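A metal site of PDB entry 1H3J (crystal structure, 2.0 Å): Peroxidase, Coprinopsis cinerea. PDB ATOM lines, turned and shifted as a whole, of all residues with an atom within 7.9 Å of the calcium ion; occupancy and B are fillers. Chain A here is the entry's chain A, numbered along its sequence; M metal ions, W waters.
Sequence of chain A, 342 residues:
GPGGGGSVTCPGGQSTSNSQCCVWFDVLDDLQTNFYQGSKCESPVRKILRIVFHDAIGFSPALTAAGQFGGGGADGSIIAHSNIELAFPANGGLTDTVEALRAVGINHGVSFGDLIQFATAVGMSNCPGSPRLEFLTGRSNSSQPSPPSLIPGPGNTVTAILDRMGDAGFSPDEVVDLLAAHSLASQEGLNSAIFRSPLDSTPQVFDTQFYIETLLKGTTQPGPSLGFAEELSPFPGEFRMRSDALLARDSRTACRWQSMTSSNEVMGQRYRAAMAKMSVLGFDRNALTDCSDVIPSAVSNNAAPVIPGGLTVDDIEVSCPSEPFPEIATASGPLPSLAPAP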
ATOM      1  N   ILE A  51      -1.185  13.306 -20.204  1.00  0.00           N
ATOM      2  CA  ILE A  51      -1.972  13.228 -21.430  1.00  0.00           C
ATOM      3  C   ILE A  51      -3.310  12.536 -21.242  1.00  0.00           C
ATOM      4  O   ILE A  51      -4.336  13.042 -21.702  1.00  0.00           O
ATOM      5  CB  ILE A  51      -1.146  12.595 -22.572  1.00  0.00           C
ATOM      6  CG1 ILE A  51      -0.013  13.552 -22.956  1.00  0.00           C
ATOM      7  CG2 ILE A  51      -2.008  12.275 -23.780  1.00  0.00           C
ATOM      8  CD1 ILE A  51       0.929  13.035 -24.008  1.00  0.00           C
ATOM      9  N   VAL A  52      -3.354  11.379 -20.612  1.00  0.00           N
ATOM     10  CA  VAL A  52      -4.639  10.731 -20.447  1.00  0.00           C
ATOM     11  C   VAL A  52      -5.656  11.599 -19.699  1.00  0.00           C
ATOM     12  O   VAL A  52      -6.830  11.701 -20.105  1.00  0.00           O
ATOM     13  CB  VAL A  52      -4.501   9.299 -19.803  1.00  0.00           C
ATOM     14  CG1 VAL A  52      -4.007   9.354 -18.360  1.00  0.00           C
ATOM     15  CG2 VAL A  52      -5.824   8.553 -19.906  1.00  0.00           C
ATOM     16  N   PHE A  53      -5.236  12.229 -18.593  1.00  0.00           N
ATOM     17  CA  PHE A  53      -6.103  13.113 -17.811  1.00  0.00           C
ATOM     18  C   PHE A  53      -6.557  14.332 -18.644  1.00  0.00           C
ATOM     19  O   PHE A  53      -7.736  14.659 -18.675  1.00  0.00           O
ATOM     20  CB  PHE A  53      -5.334  13.571 -16.549  1.00  0.00           C
ATOM     21  CG  PHE A  53      -6.052  14.604 -15.716  1.00  0.00           C
ATOM     22  CD1 PHE A  53      -5.365  15.717 -15.223  1.00  0.00           C
ATOM     23  CD2 PHE A  53      -7.421  14.483 -15.425  1.00  0.00           C
ATOM     24  CE1 PHE A  53      -6.035  16.687 -14.439  1.00  0.00           C
ATOM     25  CE2 PHE A  53      -8.090  15.429 -14.663  1.00  0.00           C
ATOM     26  CZ  PHE A  53      -7.412  16.541 -14.165  1.00  0.00           C
ATOM     27  N   HIS A  54      -5.617  14.989 -19.341  1.00  0.00           N
ATOM     28  CA  HIS A  54      -5.966  16.169 -20.149  1.00  0.00           C
ATOM     29  C   HIS A  54      -6.825  15.834 -21.376  1.00  0.00           C
ATOM     30  O   HIS A  54      -7.641  16.668 -21.797  1.00  0.00           O
ATOM     31  CB  HIS A  54      -4.708  16.974 -20.526  1.00  0.00           C
ATOM     32  CG  HIS A  54      -3.992  17.573 -19.350  1.00  0.00           C
ATOM     33  ND1 HIS A  54      -2.991  18.503 -19.484  1.00  0.00           N
ATOM     34  CD2 HIS A  54      -4.082  17.310 -18.019  1.00  0.00           C
ATOM     35  CE1 HIS A  54      -2.474  18.780 -18.302  1.00  0.00           C
ATOM     36  NE2 HIS A  54      -3.113  18.066 -17.392  1.00  0.00           N
ATOM     37  N   ASP A  55      -6.683  14.627 -21.925  1.00  0.00           N
ATOM     38  CA  ASP A  55      -7.536  14.232 -23.035  1.00  0.00           C
ATOM     39  C   ASP A  55      -8.931  13.966 -22.523  1.00  0.00           C
ATOM     40  O   ASP A  55      -9.910  14.500 -23.044  1.00  0.00           O
ATOM     41  CB  ASP A  55      -7.034  12.962 -23.726  1.00  0.00           C
ATOM     42  CG  ASP A  55      -7.984  12.499 -24.859  1.00  0.00           C
ATOM     43  OD1 ASP A  55      -8.515  13.382 -25.578  1.00  0.00           O
ATOM     44  OD2 ASP A  55      -8.205  11.283 -25.017  1.00  0.00           O
ATOM     45  N   ALA A  56      -9.045  13.120 -21.498  1.00  0.00           N
ATOM     46  CA  ALA A  56     -10.327  12.748 -20.954  1.00  0.00           C
ATOM     47  C   ALA A  56     -11.122  13.807 -20.274  1.00  0.00           C
ATOM     48  O   ALA A  56     -12.333  13.805 -20.389  1.00  0.00           O
ATOM     49  CB  ALA A  56     -10.152  11.589 -19.999  1.00  0.00           C
ATOM     50  N   ILE A  57     -10.465  14.742 -19.618  1.00  0.00           N
ATOM     51  CA  ILE A  57     -11.186  15.758 -18.862  1.00  0.00           C
ATOM     52  C   ILE A  57     -11.903  16.847 -19.702  1.00  0.00           C
ATOM     53  O   ILE A  57     -12.717  17.637 -19.162  1.00  0.00           O
ATOM     54  CB  ILE A  57     -10.274  16.362 -17.762  1.00  0.00           C
ATOM     55  CG1 ILE A  57     -11.128  16.893 -16.621  1.00  0.00           C
ATOM     56  CG2 ILE A  57      -9.357  17.426 -18.338  1.00  0.00           C
ATOM     57  CD1 ILE A  57     -11.996  15.852 -15.966  1.00  0.00           C
ATOM     58  N   GLY A  58     -11.632  16.874 -21.015  1.00  0.00           N
ATOM     59  CA  GLY A  58     -12.297  17.816 -21.904  1.00  0.00           C
ATOM     60  C   GLY A  58     -13.675  17.202 -22.166  1.00  0.00           C
ATOM     61  O   GLY A  58     -13.955  16.684 -23.266  1.00  0.00           O
ATOM     62  N   PHE A  59     -14.508  17.240 -21.140  1.00  0.00           N
ATOM     63  CA  PHE A  59     -15.825  16.645 -21.188  1.00  0.00           C
ATOM     64  C   PHE A  59     -16.643  17.420 -20.188  1.00  0.00           C
ATOM     65  O   PHE A  59     -16.245  17.531 -19.042  1.00  0.00           O
ATOM     66  CB  PHE A  59     -15.718  15.173 -20.770  1.00  0.00           C
ATOM     67  CG  PHE A  59     -17.039  14.457 -20.708  1.00  0.00           C
ATOM     68  CD1 PHE A  59     -17.699  14.083 -21.876  1.00  0.00           C
ATOM     69  CD2 PHE A  59     -17.628  14.172 -19.481  1.00  0.00           C
ATOM     70  CE1 PHE A  59     -18.927  13.445 -21.820  1.00  0.00           C
ATOM     71  CE2 PHE A  59     -18.855  13.536 -19.401  1.00  0.00           C
ATOM     72  CZ  PHE A  59     -19.510  13.166 -20.582  1.00  0.00           C
ATOM     73  N   GLY A  71     -17.248  18.796 -25.379  1.00  0.00           N
ATOM     74  CA  GLY A  71     -16.034  18.005 -25.521  1.00  0.00           C
ATOM     75  C   GLY A  71     -16.392  16.530 -25.563  1.00  0.00           C
ATOM     76  O   GLY A  71     -17.408  16.111 -24.986  1.00  0.00           O
ATOM     77  N   GLY A  72     -15.591  15.742 -26.262  1.00  0.00           N
ATOM     78  CA  GLY A  72     -15.861  14.312 -26.369  1.00  0.00           C
ATOM     79  C   GLY A  72     -15.190  13.367 -25.377  1.00  0.00           C
ATOM     80  O   GLY A  72     -15.193  12.148 -25.592  1.00  0.00           O
ATOM     81  N   GLY A  73     -14.562  13.924 -24.337  1.00  0.00           N
ATOM     82  CA  GLY A  73     -13.901  13.112 -23.326  1.00  0.00           C
ATOM     83  C   GLY A  73     -12.660  12.409 -23.806  1.00  0.00           C
ATOM     84  O   GLY A  73     -11.793  13.035 -24.452  1.00  0.00           O
ATOM     85  N   ALA A  74     -12.579  11.119 -23.483  1.00  0.00           N
ATOM     86  CA  ALA A  74     -11.444  10.258 -23.837  1.00  0.00           C
ATOM     87  C   ALA A  74     -11.433   9.824 -25.309  1.00  0.00           C
ATOM     88  O   ALA A  74     -11.250   8.648 -25.617  1.00  0.00           O
ATOM     89  CB  ALA A  74     -11.422   9.054 -22.926  1.00  0.00           C
ATOM     90  N   ASP A  75     -11.473  10.819 -26.195  1.00  0.00           N
ATOM     91  CA  ASP A  75     -11.531  10.615 -27.639  1.00  0.00           C
ATOM     92  C   ASP A  75     -10.239  10.808 -28.411  1.00  0.00           C
ATOM     93  O   ASP A  75     -10.250  10.817 -29.619  1.00  0.00           O
ATOM     94  CB  ASP A  75     -12.615  11.553 -28.201  1.00  0.00           C
ATOM     95  CG  ASP A  75     -12.329  13.046 -27.875  1.00  0.00           C
ATOM     96  OD1 ASP A  75     -13.155  13.933 -28.199  1.00  0.00           O
ATOM     97  OD2 ASP A  75     -11.251  13.344 -27.338  1.00  0.00           O
ATOM     98  N   GLY A  76      -9.123  10.998 -27.721  1.00  0.00           N
ATOM     99  CA  GLY A  76      -7.863  11.212 -28.420  1.00  0.00           C
ATOM    100  C   GLY A  76      -7.782  12.560 -29.128  1.00  0.00           C
ATOM    101  O   GLY A  76      -6.873  12.790 -29.900  1.00  0.00           O
ATOM    102  N   SER A  77      -8.711  13.481 -28.824  1.00  0.00           N
ATOM    103  CA  SER A  77      -8.712  14.825 -29.430  1.00  0.00           C
ATOM    104  C   SER A  77      -7.418  15.582 -29.225  1.00  0.00           C
ATOM    105  O   SER A  77      -7.022  16.408 -30.047  1.00  0.00           O
ATOM    106  CB  SER A  77      -9.863  15.667 -28.885  1.00  0.00           C
ATOM    107  OG  SER A  77      -9.803  15.854 -27.485  1.00  0.00           O
ATOM    108  N   ILE A  78      -6.771  15.319 -28.079  1.00  0.00           N
ATOM    109  CA  ILE A  78      -5.515  15.962 -27.742  1.00  0.00           C
ATOM    110  C   ILE A  78      -4.430  15.675 -28.792  1.00  0.00           C
ATOM    111  O   ILE A  78      -3.484  16.454 -28.968  1.00  0.00           O
ATOM    112  CB  ILE A  78      -5.072  15.593 -26.279  1.00  0.00           C
ATOM    113  CG1 ILE A  78      -3.911  16.494 -25.829  1.00  0.00           C
ATOM    114  CG2 ILE A  78      -4.653  14.139 -26.197  1.00  0.00           C
ATOM    115  CD1 ILE A  78      -3.743  16.542 -24.300  1.00  0.00           C
ATOM    116  N   ILE A  79      -4.580  14.552 -29.513  1.00  0.00           N
ATOM    117  CA  ILE A  79      -3.642  14.178 -30.578  1.00  0.00           C
ATOM    118  C   ILE A  79      -4.238  14.622 -31.932  1.00  0.00           C
ATOM    119  O   ILE A  79      -3.594  15.334 -32.678  1.00  0.00           O
ATOM    120  CB  ILE A  79      -3.342  12.643 -30.632  1.00  0.00           C
ATOM    121  CG1 ILE A  79      -2.618  12.203 -29.356  1.00  0.00           C
ATOM    122  CG2 ILE A  79      -2.444  12.312 -31.815  1.00  0.00           C
ATOM    123  CD1 ILE A  79      -2.402  10.697 -29.282  1.00  0.00           C
ATOM    124  N   HIS A  81      -6.396  16.833 -32.635  1.00  0.00           N
ATOM    125  CA  HIS A  81      -6.482  18.291 -32.700  1.00  0.00           C
ATOM    126  C   HIS A  81      -5.463  18.991 -31.823  1.00  0.00           C
ATOM    127  O   HIS A  81      -5.727  20.056 -31.288  1.00  0.00           O
ATOM    128  CB  HIS A  81      -7.872  18.711 -32.310  1.00  0.00           C
ATOM    129  CG  HIS A  81      -8.932  18.087 -33.148  1.00  0.00           C
ATOM    130  ND1 HIS A  81      -9.192  18.499 -34.440  1.00  0.00           N
ATOM    131  CD2 HIS A  81      -9.753  17.034 -32.917  1.00  0.00           C
ATOM    132  CE1 HIS A  81     -10.132  17.729 -34.968  1.00  0.00           C
ATOM    133  NE2 HIS A  81     -10.491  16.839 -34.059  1.00  0.00           N
ATOM    134  N   GLU A  85      -5.437  22.075 -29.070  1.00  0.00           N
ATOM    135  CA  GLU A  85      -5.287  21.709 -27.655  1.00  0.00           C
ATOM    136  C   GLU A  85      -3.921  21.895 -27.025  1.00  0.00           C
ATOM    137  O   GLU A  85      -3.810  22.260 -25.858  1.00  0.00           O
ATOM    138  CB  GLU A  85      -5.806  20.268 -27.432  1.00  0.00           C
ATOM    139  CG  GLU A  85      -7.259  20.108 -27.827  1.00  0.00           C
ATOM    140  CD  GLU A  85      -7.910  18.855 -27.237  1.00  0.00           C
ATOM    141  OE1 GLU A  85      -7.391  18.311 -26.227  1.00  0.00           O
ATOM    142  OE2 GLU A  85      -8.954  18.425 -27.770  1.00  0.00           O
ATOM    143  N   ILE A 116      -4.264   6.101 -26.257  1.00  0.00           N
ATOM    144  CA  ILE A 116      -3.912   6.841 -25.049  1.00  0.00           C
ATOM    145  C   ILE A 116      -4.199   6.004 -23.811  1.00  0.00           C
ATOM    146  O   ILE A 116      -3.370   5.939 -22.900  1.00  0.00           O
ATOM    147  CB  ILE A 116      -4.642   8.240 -25.001  1.00  0.00           C
ATOM    148  CG1 ILE A 116      -4.034   9.152 -26.081  1.00  0.00           C
ATOM    149  CG2 ILE A 116      -4.445   8.907 -23.621  1.00  0.00           C
ATOM    150  CD1 ILE A 116      -4.725  10.496 -26.229  1.00  0.00           C
ATOM    151  N   SER A 143     -13.076  12.798 -33.614  1.00  0.00           N
ATOM    152  CA  SER A 143     -13.261  13.670 -32.455  1.00  0.00           C
ATOM    153  C   SER A 143     -13.224  15.140 -32.878  1.00  0.00           C
ATOM    154  O   SER A 143     -12.772  15.474 -33.990  1.00  0.00           O
ATOM    155  CB  SER A 143     -12.118  13.418 -31.458  1.00  0.00           C
ATOM    156  OG  SER A 143     -10.895  13.792 -32.054  1.00  0.00           O
ATOM    157  N   GLN A 144     -13.717  16.008 -32.000  1.00  0.00           N
ATOM    158  CA  GLN A 144     -13.719  17.444 -32.213  1.00  0.00           C
ATOM    159  C   GLN A 144     -12.785  18.003 -31.143  1.00  0.00           C
ATOM    160  O   GLN A 144     -12.605  17.370 -30.084  1.00  0.00           O
ATOM    161  CB  GLN A 144     -15.108  18.021 -31.978  1.00  0.00           C
ATOM    162  CG  GLN A 144     -16.074  17.881 -33.122  1.00  0.00           C
ATOM    163  CD  GLN A 144     -17.300  18.764 -32.902  1.00  0.00           C
ATOM    164  OE1 GLN A 144     -18.392  18.276 -32.575  1.00  0.00           O
ATOM    165  NE2 GLN A 144     -17.121  20.092 -33.037  1.00  0.00           N
ATOM    166  N   PRO A 145     -12.182  19.179 -31.391  1.00  0.00           N
ATOM    167  CA  PRO A 145     -11.269  19.768 -30.405  1.00  0.00           C
ATOM    168  C   PRO A 145     -12.053  19.991 -29.120  1.00  0.00           C
ATOM    169  O   PRO A 145     -13.273  20.210 -29.134  1.00  0.00           O
ATOM    170  CB  PRO A 145     -10.898  21.119 -31.049  1.00  0.00           C
ATOM    171  CG  PRO A 145     -11.113  20.886 -32.517  1.00  0.00           C
ATOM    172  CD  PRO A 145     -12.359  20.065 -32.545  1.00  0.00           C
ATOM    173  N   SER A 146     -11.358  19.876 -27.991  1.00  0.00           N
ATOM    174  CA  SER A 146     -11.985  20.088 -26.686  1.00  0.00           C
ATOM    175  C   SER A 146     -12.191  21.588 -26.492  1.00  0.00           C
ATOM    176  O   SER A 146     -11.409  22.377 -26.995  1.00  0.00           O
ATOM    177  CB  SER A 146     -11.015  19.640 -25.590  1.00  0.00           C
ATOM    178  OG  SER A 146     -11.437  20.085 -24.314  1.00  0.00           O
ATOM    179  N   PRO A 147     -13.297  21.995 -25.826  1.00  0.00           N
ATOM    180  CA  PRO A 147     -13.477  23.417 -25.593  1.00  0.00           C
ATOM    181  C   PRO A 147     -12.331  23.822 -24.633  1.00  0.00           C
ATOM    182  O   PRO A 147     -11.746  22.943 -23.941  1.00  0.00           O
ATOM    183  CB  PRO A 147     -14.803  23.447 -24.813  1.00  0.00           C
ATOM    184  CG  PRO A 147     -15.541  22.330 -25.341  1.00  0.00           C
ATOM    185  CD  PRO A 147     -14.491  21.240 -25.428  1.00  0.00           C
ATOM    186  N   LEU A 281     -15.146   8.430 -20.288  1.00  0.00           N
ATOM    187  CA  LEU A 281     -15.919   9.681 -20.321  1.00  0.00           C
ATOM    188  C   LEU A 281     -16.155   9.954 -21.810  1.00  0.00           C
ATOM    189  O   LEU A 281     -15.205   9.952 -22.597  1.00  0.00           O
ATOM    190  CB  LEU A 281     -15.130  10.839 -19.708  1.00  0.00           C
ATOM    191  CG  LEU A 281     -14.949  10.892 -18.196  1.00  0.00           C
ATOM    192  CD1 LEU A 281     -14.133  12.137 -17.851  1.00  0.00           C
ATOM    193  CD2 LEU A 281     -16.263  10.922 -17.482  1.00  0.00           C
ATOM    194  N   PHE A 283     -18.049   7.946 -23.718  1.00  0.00           N
ATOM    195  CA  PHE A 283     -18.435   6.679 -24.346  1.00  0.00           C
ATOM    196  C   PHE A 283     -19.299   5.807 -23.438  1.00  0.00           C
ATOM    197  O   PHE A 283     -19.415   6.090 -22.243  1.00  0.00           O
ATOM    198  CB  PHE A 283     -17.186   5.889 -24.756  1.00  0.00           C
ATOM    199  CG  PHE A 283     -16.240   6.658 -25.604  1.00  0.00           C
ATOM    200  CD1 PHE A 283     -16.273   6.558 -26.984  1.00  0.00           C
ATOM    201  CD2 PHE A 283     -15.342   7.545 -25.033  1.00  0.00           C
ATOM    202  CE1 PHE A 283     -15.417   7.312 -27.790  1.00  0.00           C
ATOM    203  CE2 PHE A 283     -14.479   8.315 -25.824  1.00  0.00           C
ATOM    204  CZ  PHE A 283     -14.515   8.195 -27.211  1.00  0.00           C
HETATM  205 CA    CA M   1     -10.354  14.802 -25.391  1.00  0.00          CA
HETATM  206  O   HOH W   1     -12.006  16.264 -25.227  1.00  0.00           O
HETATM  207  O   HOH W   2      -8.819  16.594 -24.677  1.00  0.00           O
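OG of Ser 77 lies close to OE2 of Glu 85 (2.7 Å). N of Gly 73 is in hydrogen-bond range of O of Gly 58, 3.0 Å away. The side-chain carboxylate (OD2) of Asp 55 is in hydrogen-bond range of the backbone NH (N) of Gly 76.
The nearest printed residue that does not touch the calcium ion is Ala 56 (4.4 Å).
The calcium ion is bound by water W1 (2.2 Å), the side-chain carboxylate of Asp 55 (2.3 Å), the side-chain hydroxyl of Ser 77 (2.4 Å), the backbone carbonyl oxygen of Asp 55 (2.4 Å), the backbone carbonyl oxygen of Gly 73 (2.5 Å), water W2 (2.5 Å) and the side-chain carboxylate of Asp 75 (2.6 Å).
Water W2 bridges OE1 of Glu 85 (2.7 Å) and O of His 54 (3.1 Å).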
